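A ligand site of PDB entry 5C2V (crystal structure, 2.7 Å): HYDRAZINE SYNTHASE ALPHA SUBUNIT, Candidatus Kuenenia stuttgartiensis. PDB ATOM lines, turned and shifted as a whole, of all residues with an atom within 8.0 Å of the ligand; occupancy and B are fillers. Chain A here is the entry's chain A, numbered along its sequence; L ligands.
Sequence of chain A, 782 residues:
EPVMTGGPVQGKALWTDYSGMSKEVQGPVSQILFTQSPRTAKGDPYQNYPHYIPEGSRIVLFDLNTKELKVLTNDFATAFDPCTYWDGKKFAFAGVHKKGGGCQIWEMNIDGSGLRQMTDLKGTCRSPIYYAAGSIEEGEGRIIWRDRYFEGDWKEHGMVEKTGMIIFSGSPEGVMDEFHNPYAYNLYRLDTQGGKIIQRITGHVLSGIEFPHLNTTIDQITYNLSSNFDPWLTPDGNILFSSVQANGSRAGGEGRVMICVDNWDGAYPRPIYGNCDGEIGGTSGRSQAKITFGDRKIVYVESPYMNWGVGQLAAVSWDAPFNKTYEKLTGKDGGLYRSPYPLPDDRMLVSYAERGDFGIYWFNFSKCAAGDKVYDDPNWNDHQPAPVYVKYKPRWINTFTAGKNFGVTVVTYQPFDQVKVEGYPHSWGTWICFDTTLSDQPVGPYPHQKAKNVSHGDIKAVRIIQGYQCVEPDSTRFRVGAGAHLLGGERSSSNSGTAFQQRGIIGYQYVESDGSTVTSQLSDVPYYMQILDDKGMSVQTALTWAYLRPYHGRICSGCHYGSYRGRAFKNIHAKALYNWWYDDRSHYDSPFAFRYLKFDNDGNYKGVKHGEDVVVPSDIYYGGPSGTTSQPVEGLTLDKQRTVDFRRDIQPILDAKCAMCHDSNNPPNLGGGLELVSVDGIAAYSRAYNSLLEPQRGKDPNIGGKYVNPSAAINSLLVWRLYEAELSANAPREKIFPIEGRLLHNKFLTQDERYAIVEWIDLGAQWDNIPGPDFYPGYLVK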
ATOM      1  N   LYS A 460     -17.561  -6.954 -29.766  1.00  0.00           N
ATOM      2  CA  LYS A 460     -16.465  -7.638 -29.099  1.00  0.00           C
ATOM      3  C   LYS A 460     -16.629  -9.153 -29.091  1.00  0.00           C
ATOM      4  O   LYS A 460     -15.657  -9.887 -29.303  1.00  0.00           O
ATOM      5  CB  LYS A 460     -16.329  -7.122 -27.666  1.00  0.00           C
ATOM      6  CG  LYS A 460     -16.047  -5.630 -27.574  1.00  0.00           C
ATOM      7  CD  LYS A 460     -14.858  -5.236 -28.432  1.00  0.00           C
ATOM      8  CE  LYS A 460     -14.547  -3.753 -28.282  1.00  0.00           C
ATOM      9  NZ  LYS A 460     -13.427  -3.333 -29.172  1.00  0.00           N
ATOM     10  N   ALA A 461     -17.843  -9.612 -28.843  1.00  0.00           N
ATOM     11  CA  ALA A 461     -18.092 -11.048 -28.721  1.00  0.00           C
ATOM     12  C   ALA A 461     -19.517 -11.407 -29.112  1.00  0.00           C
ATOM     13  O   ALA A 461     -20.297 -10.558 -29.562  1.00  0.00           O
ATOM     14  CB  ALA A 461     -17.802 -11.507 -27.301  1.00  0.00           C
ATOM     15  N   GLN A 509     -18.243 -16.349 -27.360  1.00  0.00           N
ATOM     16  CA  GLN A 509     -17.114 -16.465 -28.271  1.00  0.00           C
ATOM     17  C   GLN A 509     -16.651 -15.090 -28.748  1.00  0.00           C
ATOM     18  O   GLN A 509     -17.467 -14.242 -29.094  1.00  0.00           O
ATOM     19  CB  GLN A 509     -17.483 -17.332 -29.474  1.00  0.00           C
ATOM     20  CG  GLN A 509     -16.293 -17.722 -30.329  1.00  0.00           C
ATOM     21  CD  GLN A 509     -15.226 -18.443 -29.522  1.00  0.00           C
ATOM     22  OE1 GLN A 509     -14.150 -17.902 -29.283  1.00  0.00           O
ATOM     23  NE2 GLN A 509     -15.538 -19.667 -29.108  1.00  0.00           N
ATOM     24  N   TYR A 510     -15.345 -14.854 -28.760  1.00  0.00           N
ATOM     25  CA  TYR A 510     -14.829 -13.547 -29.133  1.00  0.00           C
ATOM     26  C   TYR A 510     -15.011 -13.275 -30.629  1.00  0.00           C
ATOM     27  O   TYR A 510     -15.124 -14.196 -31.432  1.00  0.00           O
ATOM     28  CB  TYR A 510     -13.346 -13.410 -28.749  1.00  0.00           C
ATOM     29  CG  TYR A 510     -12.410 -14.403 -29.407  1.00  0.00           C
ATOM     30  CD1 TYR A 510     -12.104 -15.606 -28.777  1.00  0.00           C
ATOM     31  CD2 TYR A 510     -11.828 -14.137 -30.642  1.00  0.00           C
ATOM     32  CE1 TYR A 510     -11.246 -16.515 -29.370  1.00  0.00           C
ATOM     33  CE2 TYR A 510     -10.970 -15.046 -31.234  1.00  0.00           C
ATOM     34  CZ  TYR A 510     -10.679 -16.235 -30.591  1.00  0.00           C
ATOM     35  OH  TYR A 510      -9.830 -17.138 -31.171  1.00  0.00           O
ATOM     36  N   VAL A 511     -15.039 -11.990 -30.973  1.00  0.00           N
ATOM     37  CA  VAL A 511     -15.191 -11.569 -32.363  1.00  0.00           C
ATOM     38  C   VAL A 511     -13.961 -10.776 -32.811  1.00  0.00           C
ATOM     39  O   VAL A 511     -13.489  -9.894 -32.091  1.00  0.00           O
ATOM     40  CB  VAL A 511     -16.463 -10.695 -32.547  1.00  0.00           C
ATOM     41  CG1 VAL A 511     -16.509 -10.094 -33.939  1.00  0.00           C
ATOM     42  CG2 VAL A 511     -17.706 -11.534 -32.290  1.00  0.00           C
ATOM     43  N   GLU A 512     -13.455 -11.105 -33.987  1.00  0.00           N
ATOM     44  CA  GLU A 512     -12.266 -10.441 -34.521  1.00  0.00           C
ATOM     45  C   GLU A 512     -12.555  -8.983 -34.870  1.00  0.00           C
ATOM     46  O   GLU A 512     -13.715  -8.585 -35.027  1.00  0.00           O
ATOM     47  CB  GLU A 512     -11.752 -11.189 -35.762  1.00  0.00           C
ATOM     48  CG  GLU A 512     -11.495 -12.679 -35.535  1.00  0.00           C
ATOM     49  CD  GLU A 512     -10.181 -12.963 -34.838  1.00  0.00           C
ATOM     50  OE1 GLU A 512      -9.587 -12.031 -34.252  1.00  0.00           O
ATOM     51  OE2 GLU A 512      -9.727 -14.133 -34.894  1.00  0.00           O
ATOM     52  N   ASN A 579      -8.801 -19.253 -38.271  1.00  0.00           N
ATOM     53  CA  ASN A 579      -8.965 -19.808 -36.928  1.00  0.00           C
ATOM     54  C   ASN A 579      -9.825 -21.068 -36.938  1.00  0.00           C
ATOM     55  O   ASN A 579     -10.165 -21.606 -35.891  1.00  0.00           O
ATOM     56  CB  ASN A 579      -9.572 -18.767 -35.988  1.00  0.00           C
ATOM     57  CG  ASN A 579      -9.217 -19.012 -34.530  1.00  0.00           C
ATOM     58  OD1 ASN A 579      -8.221 -19.676 -34.232  1.00  0.00           O
ATOM     59  ND2 ASN A 579     -10.033 -18.483 -33.626  1.00  0.00           N
ATOM     60  N   PRO A 591     -11.893 -22.584 -31.531  1.00  0.00           N
ATOM     61  CA  PRO A 591     -12.153 -22.560 -30.082  1.00  0.00           C
ATOM     62  C   PRO A 591     -13.604 -22.871 -29.738  1.00  0.00           C
ATOM     63  O   PRO A 591     -14.511 -22.428 -30.432  1.00  0.00           O
ATOM     64  CB  PRO A 591     -11.805 -21.120 -29.688  1.00  0.00           C
ATOM     65  CG  PRO A 591     -10.904 -20.632 -30.777  1.00  0.00           C
ATOM     66  CD  PRO A 591     -11.396 -21.294 -32.019  1.00  0.00           C
ATOM     67  N   PHE A 594     -16.828 -20.326 -24.676  1.00  0.00           N
ATOM     68  CA  PHE A 594     -16.382 -20.129 -23.296  1.00  0.00           C
ATOM     69  C   PHE A 594     -17.571 -19.942 -22.361  1.00  0.00           C
ATOM     70  O   PHE A 594     -18.607 -19.408 -22.760  1.00  0.00           O
ATOM     71  CB  PHE A 594     -15.428 -18.937 -23.208  1.00  0.00           C
ATOM     72  CG  PHE A 594     -14.139 -19.116 -23.959  1.00  0.00           C
ATOM     73  CD1 PHE A 594     -14.095 -19.000 -25.333  1.00  0.00           C
ATOM     74  CD2 PHE A 594     -12.969 -19.413 -23.279  1.00  0.00           C
ATOM     75  CE1 PHE A 594     -12.912 -19.173 -26.027  1.00  0.00           C
ATOM     76  CE2 PHE A 594     -11.782 -19.580 -23.966  1.00  0.00           C
ATOM     77  CZ  PHE A 594     -11.745 -19.458 -25.340  1.00  0.00           C
ATOM     78  N   TYR A 596     -17.739 -18.131 -19.433  1.00  0.00           N
ATOM     79  CA  TYR A 596     -17.943 -16.776 -18.917  1.00  0.00           C
ATOM     80  C   TYR A 596     -17.247 -15.694 -19.723  1.00  0.00           C
ATOM     81  O   TYR A 596     -16.547 -15.967 -20.695  1.00  0.00           O
ATOM     82  CB  TYR A 596     -17.465 -16.686 -17.463  1.00  0.00           C
ATOM     83  CG  TYR A 596     -18.064 -17.707 -16.525  1.00  0.00           C
ATOM     84  CD1 TYR A 596     -19.370 -17.604 -16.078  1.00  0.00           C
ATOM     85  CD2 TYR A 596     -17.300 -18.769 -16.059  1.00  0.00           C
ATOM     86  CE1 TYR A 596     -19.909 -18.533 -15.215  1.00  0.00           C
ATOM     87  CE2 TYR A 596     -17.832 -19.705 -15.196  1.00  0.00           C
ATOM     88  CZ  TYR A 596     -19.134 -19.585 -14.777  1.00  0.00           C
ATOM     89  OH  TYR A 596     -19.666 -20.521 -13.914  1.00  0.00           O
ATOM     90  N   LEU A 597     -17.456 -14.444 -19.305  1.00  0.00           N
ATOM     91  CA  LEU A 597     -16.727 -13.300 -19.819  1.00  0.00           C
ATOM     92  C   LEU A 597     -15.996 -12.618 -18.661  1.00  0.00           C
ATOM     93  O   LEU A 597     -16.404 -12.724 -17.509  1.00  0.00           O
ATOM     94  CB  LEU A 597     -17.673 -12.296 -20.494  1.00  0.00           C
ATOM     95  CG  LEU A 597     -18.278 -12.656 -21.853  1.00  0.00           C
ATOM     96  CD1 LEU A 597     -19.181 -11.527 -22.343  1.00  0.00           C
ATOM     97  CD2 LEU A 597     -17.188 -12.931 -22.871  1.00  0.00           C
ATOM     98  N   LYS A 598     -14.897 -11.932 -18.982  1.00  0.00           N
ATOM     99  CA  LYS A 598     -14.167 -11.186 -17.967  1.00  0.00           C
ATOM    100  C   LYS A 598     -14.065  -9.713 -18.347  1.00  0.00           C
ATOM    101  O   LYS A 598     -13.849  -9.371 -19.521  1.00  0.00           O
ATOM    102  CB  LYS A 598     -12.767 -11.778 -17.764  1.00  0.00           C
ATOM    103  CG  LYS A 598     -11.869 -11.743 -18.982  1.00  0.00           C
ATOM    104  CD  LYS A 598     -10.529 -12.381 -18.697  1.00  0.00           C
ATOM    105  CE  LYS A 598      -9.629 -12.375 -19.923  1.00  0.00           C
ATOM    106  NZ  LYS A 598      -8.315 -13.027 -19.639  1.00  0.00           N
ATOM    107  N   TYR A 605     -15.868  -4.901 -21.535  1.00  0.00           N
ATOM    108  CA  TYR A 605     -15.356  -6.190 -22.003  1.00  0.00           C
ATOM    109  C   TYR A 605     -13.833  -6.240 -22.026  1.00  0.00           C
ATOM    110  O   TYR A 605     -13.171  -5.356 -22.568  1.00  0.00           O
ATOM    111  CB  TYR A 605     -15.898  -6.500 -23.408  1.00  0.00           C
ATOM    112  CG  TYR A 605     -15.313  -7.751 -24.043  1.00  0.00           C
ATOM    113  CD1 TYR A 605     -14.243  -7.675 -24.925  1.00  0.00           C
ATOM    114  CD2 TYR A 605     -15.852  -9.004 -23.778  1.00  0.00           C
ATOM    115  CE1 TYR A 605     -13.709  -8.799 -25.514  1.00  0.00           C
ATOM    116  CE2 TYR A 605     -15.325 -10.150 -24.361  1.00  0.00           C
ATOM    117  CZ  TYR A 605     -14.260 -10.033 -25.229  1.00  0.00           C
ATOM    118  OH  TYR A 605     -13.731 -11.162 -25.812  1.00  0.00           O
ATOM    119  N   LYS A 606     -13.277  -7.284 -21.424  1.00  0.00           N
ATOM    120  CA  LYS A 606     -11.842  -7.538 -21.450  1.00  0.00           C
ATOM    121  C   LYS A 606     -11.573  -8.786 -22.274  1.00  0.00           C
ATOM    122  O   LYS A 606     -10.852  -8.736 -23.278  1.00  0.00           O
ATOM    123  CB  LYS A 606     -11.278  -7.672 -20.030  1.00  0.00           C
ATOM    124  CG  LYS A 606     -10.026  -6.825 -19.791  1.00  0.00           C
ATOM    125  CD  LYS A 606     -10.144  -5.475 -20.475  1.00  0.00           C
ATOM    126  CE  LYS A 606      -8.956  -4.574 -20.155  1.00  0.00           C
ATOM    127  NZ  LYS A 606      -9.251  -3.150 -20.475  1.00  0.00           N
ATOM    128  N   GLY A 607     -12.134  -9.913 -21.857  1.00  0.00           N
ATOM    129  CA  GLY A 607     -11.921 -11.154 -22.572  1.00  0.00           C
ATOM    130  C   GLY A 607     -12.957 -12.242 -22.305  1.00  0.00           C
ATOM    131  O   GLY A 607     -13.996 -11.975 -21.709  1.00  0.00           O
ATOM    132  N   VAL A 608     -12.666 -13.450 -22.774  1.00  0.00           N
ATOM    133  CA  VAL A 608     -13.512 -14.611 -22.509  1.00  0.00           C
ATOM    134  C   VAL A 608     -12.844 -15.490 -21.463  1.00  0.00           C
ATOM    135  O   VAL A 608     -11.619 -15.565 -21.391  1.00  0.00           O
ATOM    136  CB  VAL A 608     -13.793 -15.430 -23.785  1.00  0.00           C
ATOM    137  CG1 VAL A 608     -14.559 -14.597 -24.794  1.00  0.00           C
ATOM    138  CG2 VAL A 608     -12.500 -15.939 -24.391  1.00  0.00           C
ATOM    139  N   LYS A 609     -13.648 -16.148 -20.635  1.00  0.00           N
ATOM    140  CA  LYS A 609     -13.094 -16.939 -19.534  1.00  0.00           C
ATOM    141  C   LYS A 609     -13.637 -18.367 -19.508  1.00  0.00           C
ATOM    142  O   LYS A 609     -14.845 -18.602 -19.540  1.00  0.00           O
ATOM    143  CB  LYS A 609     -13.379 -16.256 -18.200  1.00  0.00           C
ATOM    144  CG  LYS A 609     -12.749 -16.939 -17.003  1.00  0.00           C
ATOM    145  CD  LYS A 609     -13.031 -16.181 -15.713  1.00  0.00           C
ATOM    146  CE  LYS A 609     -12.361 -16.851 -14.535  1.00  0.00           C
ATOM    147  NZ  LYS A 609     -12.615 -16.108 -13.264  1.00  0.00           N
ATOM    148  N   HIS A 610     -12.703 -19.315 -19.429  1.00  0.00           N
ATOM    149  CA  HIS A 610     -13.018 -20.738 -19.361  1.00  0.00           C
ATOM    150  C   HIS A 610     -13.826 -21.109 -18.125  1.00  0.00           C
ATOM    151  O   HIS A 610     -13.648 -20.529 -17.051  1.00  0.00           O
ATOM    152  CB  HIS A 610     -11.742 -21.580 -19.368  1.00  0.00           C
ATOM    153  CG  HIS A 610     -11.148 -21.779 -20.730  1.00  0.00           C
ATOM    154  ND1 HIS A 610     -11.752 -22.573 -21.687  1.00  0.00           N
ATOM    155  CD2 HIS A 610     -10.005 -21.320 -21.280  1.00  0.00           C
ATOM    156  CE1 HIS A 610     -11.001 -22.573 -22.780  1.00  0.00           C
ATOM    157  NE2 HIS A 610      -9.944 -21.827 -22.559  1.00  0.00           N
HETATM  158  N1  LIG L   1      -8.139 -13.348 -26.845  1.00  0.00           N
HETATM  159  C1  LIG L   1      -8.555 -12.564 -25.605  1.00  0.00           C
HETATM  160  C2  LIG L   1     -10.127 -12.804 -25.299  1.00  0.00           C
HETATM  161  O1  LIG L   1     -10.917 -12.253 -26.100  1.00  0.00           O
HETATM  162  O2  LIG L   1     -10.332 -13.508 -24.276  1.00  0.00           O
HETATM  163  C3  LIG L   1      -8.910 -14.653 -26.955  1.00  0.00           C
HETATM  164  C4  LIG L   1      -6.651 -13.700 -26.773  1.00  0.00           C
HETATM  165  C5  LIG L   1      -8.433 -12.562 -28.106  1.00  0.00           C
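N of Lys 598 is in hydrogen-bond range of O of Gly 607. The side-chain hydroxyl (OH) of Tyr 510 sits at hydrogen-bond distance from the side-chain amide nitrogen (ND2) of Asn 579, 2.8 Å away.
CB of Tyr 510 touches O1 of the ligand, 3.8 Å away. Gly 607 touches the ligand (CA to O2, 3.3 Å). Hydrophobic or aromatic side chains that line the ligand: Tyr 510 and Val 608. Of the 18 residues printed, 4 come within 4 Å of the ligand.
An oxygen (O1) of the ligand is in hydrogen-bond range of the side-chain hydroxyl of Tyr 605 (3.0 Å). N of Val 608 sits at hydrogen-bond distance from O2 of the ligand, 2.8 Å away.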
